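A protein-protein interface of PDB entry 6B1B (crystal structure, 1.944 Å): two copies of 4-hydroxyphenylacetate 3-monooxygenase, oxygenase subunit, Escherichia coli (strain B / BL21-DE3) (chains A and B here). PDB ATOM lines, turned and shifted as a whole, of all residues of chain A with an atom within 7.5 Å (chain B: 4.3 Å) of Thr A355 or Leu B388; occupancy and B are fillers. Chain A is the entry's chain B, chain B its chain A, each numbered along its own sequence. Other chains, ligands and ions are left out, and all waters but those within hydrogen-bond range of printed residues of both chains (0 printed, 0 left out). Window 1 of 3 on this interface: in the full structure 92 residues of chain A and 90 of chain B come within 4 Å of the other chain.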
ATOM      1  N   CYS A 313     -11.952 -28.605 -38.295  1.00  0.00           N
ATOM      2  CA  CYS A 313     -13.067 -28.194 -37.446  1.00  0.00           C
ATOM      3  C   CYS A 313     -14.173 -27.545 -38.268  1.00  0.00           C
ATOM      4  O   CYS A 313     -15.360 -27.821 -38.051  1.00  0.00           O
ATOM      5  CB  CYS A 313     -12.574 -27.228 -36.363  1.00  0.00           C
ATOM      6  SG  CYS A 313     -13.862 -26.757 -35.139  1.00  0.00           S
ATOM      7  N   ALA A 317     -17.997 -28.785 -38.864  1.00  0.00           N
ATOM      8  CA  ALA A 317     -19.120 -27.906 -38.533  1.00  0.00           C
ATOM      9  C   ALA A 317     -20.109 -27.797 -39.691  1.00  0.00           C
ATOM     10  O   ALA A 317     -21.327 -27.757 -39.476  1.00  0.00           O
ATOM     11  CB  ALA A 317     -18.596 -26.527 -38.120  1.00  0.00           C
ATOM     12  N   LEU A 320     -22.078 -30.860 -39.712  1.00  0.00           N
ATOM     13  CA  LEU A 320     -23.101 -30.831 -38.661  1.00  0.00           C
ATOM     14  C   LEU A 320     -24.248 -29.879 -39.013  1.00  0.00           C
ATOM     15  O   LEU A 320     -25.387 -30.124 -38.605  1.00  0.00           O
ATOM     16  CB  LEU A 320     -22.469 -30.458 -37.312  1.00  0.00           C
ATOM     17  CG  LEU A 320     -21.427 -31.481 -36.811  1.00  0.00           C
ATOM     18  CD1 LEU A 320     -20.922 -31.168 -35.399  1.00  0.00           C
ATOM     19  CD2 LEU A 320     -21.980 -32.906 -36.867  1.00  0.00           C
ATOM     20  N   GLU A 348     -30.274 -30.554 -28.762  1.00  0.00           N
ATOM     21  CA  GLU A 348     -28.921 -30.949 -28.387  1.00  0.00           C
ATOM     22  C   GLU A 348     -28.023 -31.091 -29.614  1.00  0.00           C
ATOM     23  O   GLU A 348     -26.836 -30.744 -29.563  1.00  0.00           O
ATOM     24  CB  GLU A 348     -28.910 -32.259 -27.591  1.00  0.00           C
ATOM     25  CG  GLU A 348     -27.472 -32.587 -27.207  1.00  0.00           C
ATOM     26  CD  GLU A 348     -27.303 -33.708 -26.206  1.00  0.00           C
ATOM     27  OE1 GLU A 348     -28.229 -33.953 -25.413  1.00  0.00           O
ATOM     28  OE2 GLU A 348     -26.212 -34.321 -26.205  1.00  0.00           O
ATOM     29  N   VAL A 349     -28.558 -31.623 -30.714  1.00  0.00           N
ATOM     30  CA  VAL A 349     -27.770 -31.687 -31.944  1.00  0.00           C
ATOM     31  C   VAL A 349     -27.359 -30.283 -32.377  1.00  0.00           C
ATOM     32  O   VAL A 349     -26.207 -30.045 -32.771  1.00  0.00           O
ATOM     33  CB  VAL A 349     -28.557 -32.426 -33.045  1.00  0.00           C
ATOM     34  CG1 VAL A 349     -27.790 -32.403 -34.372  1.00  0.00           C
ATOM     35  CG2 VAL A 349     -28.819 -33.875 -32.629  1.00  0.00           C
ATOM     36  N   VAL A 350     -28.294 -29.332 -32.302  1.00  0.00           N
ATOM     37  CA  VAL A 350     -27.973 -27.934 -32.590  1.00  0.00           C
ATOM     38  C   VAL A 350     -26.837 -27.442 -31.698  1.00  0.00           C
ATOM     39  O   VAL A 350     -25.917 -26.739 -32.162  1.00  0.00           O
ATOM     40  CB  VAL A 350     -29.227 -27.048 -32.430  1.00  0.00           C
ATOM     41  CG1 VAL A 350     -28.830 -25.563 -32.543  1.00  0.00           C
ATOM     42  CG2 VAL A 350     -30.292 -27.408 -33.469  1.00  0.00           C
ATOM     43  N   ALA A 351     -26.889 -27.769 -30.396  1.00  0.00           N
ATOM     44  CA  ALA A 351     -25.826 -27.328 -29.490  1.00  0.00           C
ATOM     45  C   ALA A 351     -24.462 -27.892 -29.905  1.00  0.00           C
ATOM     46  O   ALA A 351     -23.448 -27.182 -29.858  1.00  0.00           O
ATOM     47  CB  ALA A 351     -26.156 -27.726 -28.045  1.00  0.00           C
ATOM     48  N   TRP A 352     -24.405 -29.175 -30.292  1.00  0.00           N
ATOM     49  CA  TRP A 352     -23.135 -29.733 -30.761  1.00  0.00           C
ATOM     50  C   TRP A 352     -22.678 -29.039 -32.035  1.00  0.00           C
ATOM     51  O   TRP A 352     -21.513 -28.666 -32.159  1.00  0.00           O
ATOM     52  CB  TRP A 352     -23.261 -31.245 -30.991  1.00  0.00           C
ATOM     53  CG  TRP A 352     -23.356 -32.016 -29.689  1.00  0.00           C
ATOM     54  CD1 TRP A 352     -24.417 -32.750 -29.243  1.00  0.00           C
ATOM     55  CD2 TRP A 352     -22.343 -32.117 -28.679  1.00  0.00           C
ATOM     56  NE1 TRP A 352     -24.130 -33.293 -28.004  1.00  0.00           N
ATOM     57  CE2 TRP A 352     -22.859 -32.923 -27.644  1.00  0.00           C
ATOM     58  CE3 TRP A 352     -21.050 -31.594 -28.547  1.00  0.00           C
ATOM     59  CZ2 TRP A 352     -22.125 -33.221 -26.489  1.00  0.00           C
ATOM     60  CZ3 TRP A 352     -20.321 -31.900 -27.404  1.00  0.00           C
ATOM     61  CH2 TRP A 352     -20.864 -32.701 -26.393  1.00  0.00           C
ATOM     62  N   ARG A 353     -23.592 -28.835 -32.982  1.00  0.00           N
ATOM     63  CA  ARG A 353     -23.268 -28.076 -34.189  1.00  0.00           C
ATOM     64  C   ARG A 353     -22.716 -26.691 -33.843  1.00  0.00           C
ATOM     65  O   ARG A 353     -21.671 -26.275 -34.368  1.00  0.00           O
ATOM     66  CB  ARG A 353     -24.524 -27.983 -35.067  1.00  0.00           C
ATOM     67  CG  ARG A 353     -24.425 -27.016 -36.216  1.00  0.00           C
ATOM     68  CD  ARG A 353     -25.032 -25.652 -35.882  1.00  0.00           C
ATOM     69  NE  ARG A 353     -24.898 -24.756 -37.025  1.00  0.00           N
ATOM     70  CZ  ARG A 353     -24.787 -23.436 -36.947  1.00  0.00           C
ATOM     71  NH1 ARG A 353     -24.789 -22.822 -35.764  1.00  0.00           N
ATOM     72  NH2 ARG A 353     -24.677 -22.727 -38.065  1.00  0.00           N
ATOM     73  N   ASN A 354     -23.388 -25.982 -32.926  1.00  0.00           N
ATOM     74  CA  ASN A 354     -22.936 -24.655 -32.496  1.00  0.00           C
ATOM     75  C   ASN A 354     -21.533 -24.702 -31.909  1.00  0.00           C
ATOM     76  O   ASN A 354     -20.766 -23.739 -32.034  1.00  0.00           O
ATOM     77  CB  ASN A 354     -23.853 -24.084 -31.407  1.00  0.00           C
ATOM     78  CG  ASN A 354     -25.239 -23.698 -31.899  1.00  0.00           C
ATOM     79  OD1 ASN A 354     -25.504 -23.596 -33.097  1.00  0.00           O
ATOM     80  ND2 ASN A 354     -26.128 -23.435 -30.944  1.00  0.00           N
ATOM     81  N   THR A 355     -21.236 -25.768 -31.161  1.00  0.00           N
ATOM     82  CA  THR A 355     -19.963 -25.898 -30.466  1.00  0.00           C
ATOM     83  C   THR A 355     -18.785 -25.804 -31.430  1.00  0.00           C
ATOM     84  O   THR A 355     -17.797 -25.116 -31.148  1.00  0.00           O
ATOM     85  CB  THR A 355     -19.926 -27.227 -29.698  1.00  0.00           C
ATOM     86  OG1 THR A 355     -20.983 -27.248 -28.732  1.00  0.00           O
ATOM     87  CG2 THR A 355     -18.582 -27.418 -29.002  1.00  0.00           C
ATOM     88  N   PHE A 356     -18.849 -26.516 -32.557  1.00  0.00           N
ATOM     89  CA  PHE A 356     -17.690 -26.532 -33.449  1.00  0.00           C
ATOM     90  C   PHE A 356     -17.545 -25.228 -34.214  1.00  0.00           C
ATOM     91  O   PHE A 356     -16.414 -24.784 -34.439  1.00  0.00           O
ATOM     92  CB  PHE A 356     -17.771 -27.775 -34.347  1.00  0.00           C
ATOM     93  CG  PHE A 356     -17.603 -29.025 -33.529  1.00  0.00           C
ATOM     94  CD1 PHE A 356     -16.339 -29.404 -33.094  1.00  0.00           C
ATOM     95  CD2 PHE A 356     -18.710 -29.712 -33.047  1.00  0.00           C
ATOM     96  CE1 PHE A 356     -16.170 -30.514 -32.264  1.00  0.00           C
ATOM     97  CE2 PHE A 356     -18.552 -30.818 -32.227  1.00  0.00           C
ATOM     98  CZ  PHE A 356     -17.290 -31.214 -31.826  1.00  0.00           C
ATOM     99  N   TRP A 357     -18.648 -24.546 -34.532  1.00  0.00           N
ATOM    100  CA  TRP A 357     -18.510 -23.184 -35.045  1.00  0.00           C
ATOM    101  C   TRP A 357     -17.866 -22.276 -34.006  1.00  0.00           C
ATOM    102  O   TRP A 357     -16.991 -21.467 -34.336  1.00  0.00           O
ATOM    103  CB  TRP A 357     -19.870 -22.623 -35.483  1.00  0.00           C
ATOM    104  CG  TRP A 357     -20.333 -23.228 -36.777  1.00  0.00           C
ATOM    105  CD1 TRP A 357     -21.402 -24.063 -36.968  1.00  0.00           C
ATOM    106  CD2 TRP A 357     -19.721 -23.053 -38.064  1.00  0.00           C
ATOM    107  NE1 TRP A 357     -21.486 -24.423 -38.299  1.00  0.00           N
ATOM    108  CE2 TRP A 357     -20.468 -23.812 -38.989  1.00  0.00           C
ATOM    109  CE3 TRP A 357     -18.613 -22.320 -38.520  1.00  0.00           C
ATOM    110  CZ2 TRP A 357     -20.139 -23.871 -40.354  1.00  0.00           C
ATOM    111  CZ3 TRP A 357     -18.288 -22.375 -39.878  1.00  0.00           C
ATOM    112  CH2 TRP A 357     -19.052 -23.146 -40.777  1.00  0.00           C
ATOM    113  N   ALA A 358     -18.268 -22.405 -32.738  1.00  0.00           N
ATOM    114  CA  ALA A 358     -17.697 -21.537 -31.706  1.00  0.00           C
ATOM    115  C   ALA A 358     -16.213 -21.813 -31.509  1.00  0.00           C
ATOM    116  O   ALA A 358     -15.431 -20.883 -31.264  1.00  0.00           O
ATOM    117  CB  ALA A 358     -18.444 -21.706 -30.378  1.00  0.00           C
ATOM    118  N   LEU A 359     -15.811 -23.086 -31.576  1.00  0.00           N
ATOM    119  CA  LEU A 359     -14.394 -23.406 -31.468  1.00  0.00           C
ATOM    120  C   LEU A 359     -13.611 -22.758 -32.606  1.00  0.00           C
ATOM    121  O   LEU A 359     -12.527 -22.211 -32.391  1.00  0.00           O
ATOM    122  CB  LEU A 359     -14.188 -24.930 -31.469  1.00  0.00           C
ATOM    123  CG  LEU A 359     -14.554 -25.632 -30.153  1.00  0.00           C
ATOM    124  CD1 LEU A 359     -14.454 -27.152 -30.317  1.00  0.00           C
ATOM    125  CD2 LEU A 359     -13.607 -25.153 -29.070  1.00  0.00           C
ATOM    126  N   SER A 360     -14.158 -22.788 -33.818  1.00  0.00           N
ATOM    127  CA  SER A 360     -13.450 -22.150 -34.925  1.00  0.00           C
ATOM    128  C   SER A 360     -13.407 -20.630 -34.751  1.00  0.00           C
ATOM    129  O   SER A 360     -12.418 -20.006 -35.150  1.00  0.00           O
ATOM    130  CB  SER A 360     -14.081 -22.564 -36.268  1.00  0.00           C
ATOM    131  OG  SER A 360     -15.282 -21.860 -36.550  1.00  0.00           O
ATOM    132  N   ASP A 361     -14.450 -20.026 -34.149  1.00  0.00           N
ATOM    133  CA  ASP A 361     -14.390 -18.611 -33.767  1.00  0.00           C
ATOM    134  C   ASP A 361     -13.213 -18.340 -32.838  1.00  0.00           C
ATOM    135  O   ASP A 361     -12.453 -17.389 -33.040  1.00  0.00           O
ATOM    136  CB  ASP A 361     -15.677 -18.158 -33.051  1.00  0.00           C
ATOM    137  CG  ASP A 361     -16.894 -18.152 -33.939  1.00  0.00           C
ATOM    138  OD1 ASP A 361     -16.761 -18.051 -35.184  1.00  0.00           O
ATOM    139  OD2 ASP A 361     -18.008 -18.226 -33.368  1.00  0.00           O
ATOM    140  N   THR A 384      -9.106 -29.023 -28.286  1.00  0.00           N
ATOM    141  CA  THR A 384     -10.461 -29.243 -27.778  1.00  0.00           C
ATOM    142  C   THR A 384     -11.376 -29.796 -28.857  1.00  0.00           C
ATOM    143  O   THR A 384     -12.180 -30.705 -28.605  1.00  0.00           O
ATOM    144  CB  THR A 384     -11.022 -27.925 -27.254  1.00  0.00           C
ATOM    145  OG1 THR A 384     -10.134 -27.422 -26.259  1.00  0.00           O
ATOM    146  CG2 THR A 384     -12.406 -28.112 -26.675  1.00  0.00           C
ATOM    147  N   TYR A 385     -11.310 -29.212 -30.056  1.00  0.00           N
ATOM    148  CA  TYR A 385     -12.066 -29.755 -31.177  1.00  0.00           C
ATOM    149  C   TYR A 385     -11.769 -31.239 -31.356  1.00  0.00           C
ATOM    150  O   TYR A 385     -12.677 -32.043 -31.577  1.00  0.00           O
ATOM    151  CB  TYR A 385     -11.744 -28.965 -32.462  1.00  0.00           C
ATOM    152  CG  TYR A 385     -11.630 -29.861 -33.673  1.00  0.00           C
ATOM    153  CD1 TYR A 385     -12.765 -30.392 -34.283  1.00  0.00           C
ATOM    154  CD2 TYR A 385     -10.385 -30.221 -34.171  1.00  0.00           C
ATOM    155  CE1 TYR A 385     -12.654 -31.258 -35.371  1.00  0.00           C
ATOM    156  CE2 TYR A 385     -10.266 -31.078 -35.251  1.00  0.00           C
ATOM    157  CZ  TYR A 385     -11.401 -31.591 -35.845  1.00  0.00           C
ATOM    158  OH  TYR A 385     -11.271 -32.442 -36.920  1.00  0.00           O
ATOM    159  N   LEU A 388     -13.446 -33.291 -28.489  1.00  0.00           N
ATOM    160  CA  LEU A 388     -14.906 -33.260 -28.470  1.00  0.00           C
ATOM    161  C   LEU A 388     -15.534 -33.924 -29.684  1.00  0.00           C
ATOM    162  O   LEU A 388     -16.624 -34.499 -29.562  1.00  0.00           O
ATOM    163  CB  LEU A 388     -15.412 -31.819 -28.389  1.00  0.00           C
ATOM    164  CG  LEU A 388     -15.208 -31.056 -27.080  1.00  0.00           C
ATOM    165  CD1 LEU A 388     -16.035 -29.765 -27.106  1.00  0.00           C
ATOM    166  CD2 LEU A 388     -15.583 -31.911 -25.881  1.00  0.00           C
ATOM    167  N   ALA A 392     -19.134 -35.905 -29.777  1.00  0.00           N
ATOM    168  CA  ALA A 392     -20.276 -35.239 -30.394  1.00  0.00           C
ATOM    169  C   ALA A 392     -20.857 -36.076 -31.526  1.00  0.00           C
ATOM    170  O   ALA A 392     -22.078 -36.222 -31.644  1.00  0.00           O
ATOM    171  CB  ALA A 392     -19.855 -33.864 -30.911  1.00  0.00           C
ATOM    172  N   THR B 355     -13.287 -25.686 -23.391  1.00  0.00           N
ATOM    173  CA  THR B 355     -14.542 -25.453 -24.110  1.00  0.00           C
ATOM    174  C   THR B 355     -15.242 -24.195 -23.627  1.00  0.00           C
ATOM    175  O   THR B 355     -15.755 -23.412 -24.437  1.00  0.00           O
ATOM    176  CB  THR B 355     -15.494 -26.659 -23.956  1.00  0.00           C
ATOM    177  OG1 THR B 355     -14.859 -27.847 -24.447  1.00  0.00           O
ATOM    178  CG2 THR B 355     -16.822 -26.443 -24.730  1.00  0.00           C
ATOM    179  N   PHE B 356     -15.326 -24.012 -22.303  1.00  0.00           N
ATOM    180  CA  PHE B 356     -16.095 -22.877 -21.818  1.00  0.00           C
ATOM    181  C   PHE B 356     -15.347 -21.566 -22.002  1.00  0.00           C
ATOM    182  O   PHE B 356     -15.981 -20.539 -22.279  1.00  0.00           O
ATOM    183  CB  PHE B 356     -16.535 -23.145 -20.370  1.00  0.00           C
ATOM    184  CG  PHE B 356     -17.523 -24.258 -20.312  1.00  0.00           C
ATOM    185  CD1 PHE B 356     -18.851 -24.034 -20.669  1.00  0.00           C
ATOM    186  CD2 PHE B 356     -17.095 -25.563 -20.096  1.00  0.00           C
ATOM    187  CE1 PHE B 356     -19.766 -25.091 -20.712  1.00  0.00           C
ATOM    188  CE2 PHE B 356     -18.002 -26.624 -20.137  1.00  0.00           C
ATOM    189  CZ  PHE B 356     -19.325 -26.395 -20.453  1.00  0.00           C
ATOM    190  N   THR B 384     -25.456 -22.572 -26.183  1.00  0.00           N
ATOM    191  CA  THR B 384     -24.582 -23.740 -26.198  1.00  0.00           C
ATOM    192  C   THR B 384     -23.943 -23.964 -24.837  1.00  0.00           C
ATOM    193  O   THR B 384     -23.876 -25.101 -24.349  1.00  0.00           O
ATOM    194  CB  THR B 384     -23.502 -23.550 -27.259  1.00  0.00           C
ATOM    195  OG1 THR B 384     -24.130 -23.306 -28.512  1.00  0.00           O
ATOM    196  CG2 THR B 384     -22.600 -24.784 -27.355  1.00  0.00           C
ATOM    197  N   TYR B 385     -23.435 -22.888 -24.226  1.00  0.00           N
ATOM    198  CA  TYR B 385     -22.917 -22.990 -22.871  1.00  0.00           C
ATOM    199  C   TYR B 385     -23.956 -23.612 -21.937  1.00  0.00           C
ATOM    200  O   TYR B 385     -23.633 -24.488 -21.131  1.00  0.00           O
ATOM    201  CB  TYR B 385     -22.493 -21.603 -22.374  1.00  0.00           C
ATOM    202  CG  TYR B 385     -22.820 -21.387 -20.928  1.00  0.00           C
ATOM    203  CD1 TYR B 385     -22.057 -21.989 -19.926  1.00  0.00           C
ATOM    204  CD2 TYR B 385     -23.909 -20.612 -20.555  1.00  0.00           C
ATOM    205  CE1 TYR B 385     -22.379 -21.817 -18.576  1.00  0.00           C
ATOM    206  CE2 TYR B 385     -24.232 -20.437 -19.213  1.00  0.00           C
ATOM    207  CZ  TYR B 385     -23.470 -21.041 -18.238  1.00  0.00           C
ATOM    208  OH  TYR B 385     -23.803 -20.862 -16.913  1.00  0.00           O
ATOM    209  N   ARG B 386     -25.221 -23.193 -22.052  1.00  0.00           N
ATOM    210  CA  ARG B 386     -26.230 -23.701 -21.124  1.00  0.00           C
ATOM    211  C   ARG B 386     -26.473 -25.191 -21.316  1.00  0.00           C
ATOM    212  O   ARG B 386     -26.680 -25.916 -20.338  1.00  0.00           O
ATOM    213  CB  ARG B 386     -27.548 -22.949 -21.263  1.00  0.00           C
ATOM    214  CG  ARG B 386     -27.561 -21.613 -20.580  1.00  0.00           C
ATOM    215  CD  ARG B 386     -29.011 -21.180 -20.343  1.00  0.00           C
ATOM    216  NE  ARG B 386     -29.631 -20.497 -21.463  1.00  0.00           N
ATOM    217  CZ  ARG B 386     -29.789 -19.181 -21.502  1.00  0.00           C
ATOM    218  NH1 ARG B 386     -29.365 -18.444 -20.484  1.00  0.00           N
ATOM    219  NH2 ARG B 386     -30.367 -18.599 -22.545  1.00  0.00           N
ATOM    220  N   VAL B 387     -26.464 -25.667 -22.562  1.00  0.00           N
ATOM    221  CA  VAL B 387     -26.677 -27.095 -22.804  1.00  0.00           C
ATOM    222  C   VAL B 387     -25.455 -27.908 -22.387  1.00  0.00           C
ATOM    223  O   VAL B 387     -25.582 -28.997 -21.807  1.00  0.00           O
ATOM    224  CB  VAL B 387     -27.026 -27.331 -24.285  1.00  0.00           C
ATOM    225  CG1 VAL B 387     -27.043 -28.827 -24.602  1.00  0.00           C
ATOM    226  CG2 VAL B 387     -28.344 -26.677 -24.631  1.00  0.00           C
ATOM    227  N   LEU B 388     -24.248 -27.408 -22.686  1.00  0.00           N
ATOM    228  CA  LEU B 388     -23.041 -28.201 -22.438  1.00  0.00           C
ATOM    229  C   LEU B 388     -22.656 -28.253 -20.966  1.00  0.00           C
ATOM    230  O   LEU B 388     -22.125 -29.273 -20.512  1.00  0.00           O
ATOM    231  CB  LEU B 388     -21.852 -27.657 -23.236  1.00  0.00           C
ATOM    232  CG  LEU B 388     -21.883 -27.863 -24.746  1.00  0.00           C
ATOM    233  CD1 LEU B 388     -20.519 -27.541 -25.361  1.00  0.00           C
ATOM    234  CD2 LEU B 388     -22.291 -29.300 -25.072  1.00  0.00           C
ATOM    235  N   ALA B 389     -22.865 -27.164 -20.218  1.00  0.00           N
ATOM    236  CA  ALA B 389     -22.366 -27.105 -18.842  1.00  0.00           C
ATOM    237  C   ALA B 389     -22.821 -28.277 -17.977  1.00  0.00           C
ATOM    238  O   ALA B 389     -21.978 -28.850 -17.267  1.00  0.00           O
ATOM    239  CB  ALA B 389     -22.765 -25.768 -18.195  1.00  0.00           C
ATOM    240  N   PRO B 390     -24.105 -28.676 -17.962  1.00  0.00           N
ATOM    241  CA  PRO B 390     -24.491 -29.812 -17.101  1.00  0.00           C
ATOM    242  C   PRO B 390     -23.796 -31.106 -17.474  1.00  0.00           C
ATOM    243  O   PRO B 390     -23.423 -31.886 -16.594  1.00  0.00           O
ATOM    244  CB  PRO B 390     -26.010 -29.907 -17.311  1.00  0.00           C
ATOM    245  CG  PRO B 390     -26.418 -28.498 -17.742  1.00  0.00           C
ATOM    246  CD  PRO B 390     -25.278 -28.093 -18.639  1.00  0.00           C
ATOM    247  N   MET B 391     -23.630 -31.366 -18.770  1.00  0.00           N
ATOM    248  CA  MET B 391     -22.961 -32.591 -19.194  1.00  0.00           C
ATOM    249  C   MET B 391     -21.486 -32.561 -18.824  1.00  0.00           C
ATOM    250  O   MET B 391     -20.934 -33.566 -18.360  1.00  0.00           O
ATOM    251  CB  MET B 391     -23.148 -32.789 -20.703  1.00  0.00           C
ATOM    252  CG  MET B 391     -24.586 -33.129 -21.093  1.00  0.00           C
ATOM    253  SD  MET B 391     -24.807 -33.597 -22.833  1.00  0.00           S
ATOM    254  CE  MET B 391     -24.521 -32.035 -23.666  1.00  0.00           C
ATOM    255  N   ALA B 392     -20.832 -31.417 -19.026  1.00  0.00           N
ATOM    256  CA  ALA B 392     -19.421 -31.296 -18.682  1.00  0.00           C
ATOM    257  C   ALA B 392     -19.196 -31.471 -17.188  1.00  0.00           C
ATOM    258  O   ALA B 392     -18.273 -32.181 -16.769  1.00  0.00           O
ATOM    259  CB  ALA B 392     -18.886 -29.932 -19.132  1.00  0.00           C
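The side-chain carboxylate (OE2) of Glu A348 lies within hydrogen-bond range of the indole nitrogen (NE1) of Trp A352 (2.9 Å).
The side-chain amide oxygen of Asn A354 sits close to the backbone carbonyl oxygen of Val A350, 3.3 Å away.
The side-chain hydroxyl (OG1) of Thr A355 lies within hydrogen-bond range of the backbone carbonyl oxygen (O) of Ala A351 (2.7 Å).
The guanidinium group (NH1) of Arg A353 is in hydrogen-bond range of the side-chain amide oxygen (OD1) of Asn A354, 2.9 Å away.
Of the 11 printed residues of chain B, 5 touch a printed residue of chain A.
Printed residues of chain B that touch a printed residue of chain A: Thr B355, Thr B384, Val B387, Leu B388 and Met B391.
Hydrophobic or aromatic side chains of chain B within 4 Å of the printed part of chain A: Val B387, Leu B388 and Met B391.
Along chain B the printed residues that touch a printed residue of chain A span positions 355 to 391.
Along chain A the printed residues that touch a printed residue of chain B span positions 348 to 388.
Among the printed residues, 10 pairs touch across the chains.
The side-chain hydroxyl (OG1) of Thr B384 lies close to the side-chain amide nitrogen (ND2) of Asn A354 (3.2 Å).
OE2 of Glu A348 sits close to SD of Met B391 (3.7 Å).
Of the printed residues of chain B, Glu A348 touches Met B391.
Thr A355 touches just these residues of chain B: Thr B384 (3.3 Å) and Leu B388 (3.4 Å).
Asp A361 touches none of the printed residues of chain B.
Tyr A385 touches none of the printed residues of chain B.
Printed residues of chain A within 4 Å of Thr B355: Thr A384 and Leu A388.
Of chain A, only Trp A352 (3.9 Å) and Thr A355 (3.4 Å) come within 4 Å of Leu B388.
The nearest printed residue of chain B that does not touch Thr A355 is Thr B355 (4.7 Å).
The nearest residue of chain A that does not touch Leu B388 is Ala A351 (5.1 Å).
The nearest printed residue of chain B that does not touch Asn A354 is Leu B388 (7.2 Å).
Thr A355 touches Thr B384, and with the chains exchanged Thr A384 touches Thr B355.
Thr A355 touches Leu B388, and with the chains exchanged Leu A388 touches Thr B355.
Positions printed for both chains: 355, 356, 384, 385, 388 and 392.
Of the 10 pairs that touch across the chains among the printed residues, 4 have their exchanged pair printed and touching as well.
O of Ala A351 touches CG2 of Thr B384, 3.6 Å away.
Val B387 touches Ala A351.
Trp A352 touches Leu B388 (CH2 to CD2, 3.9 Å).
Trp A352 touches Met B391 (CZ2 to CE, 3.9 Å).
Thr B384 touches Thr A355 (CG2 to OG1, 3.3 Å).
Thr A355 touches Leu B388 (OG1 to CD1, 3.4 Å).
Thr A384 touches Thr B355 (CG2 to OG1, 3.3 Å).
Thr B355 touches Leu A388.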
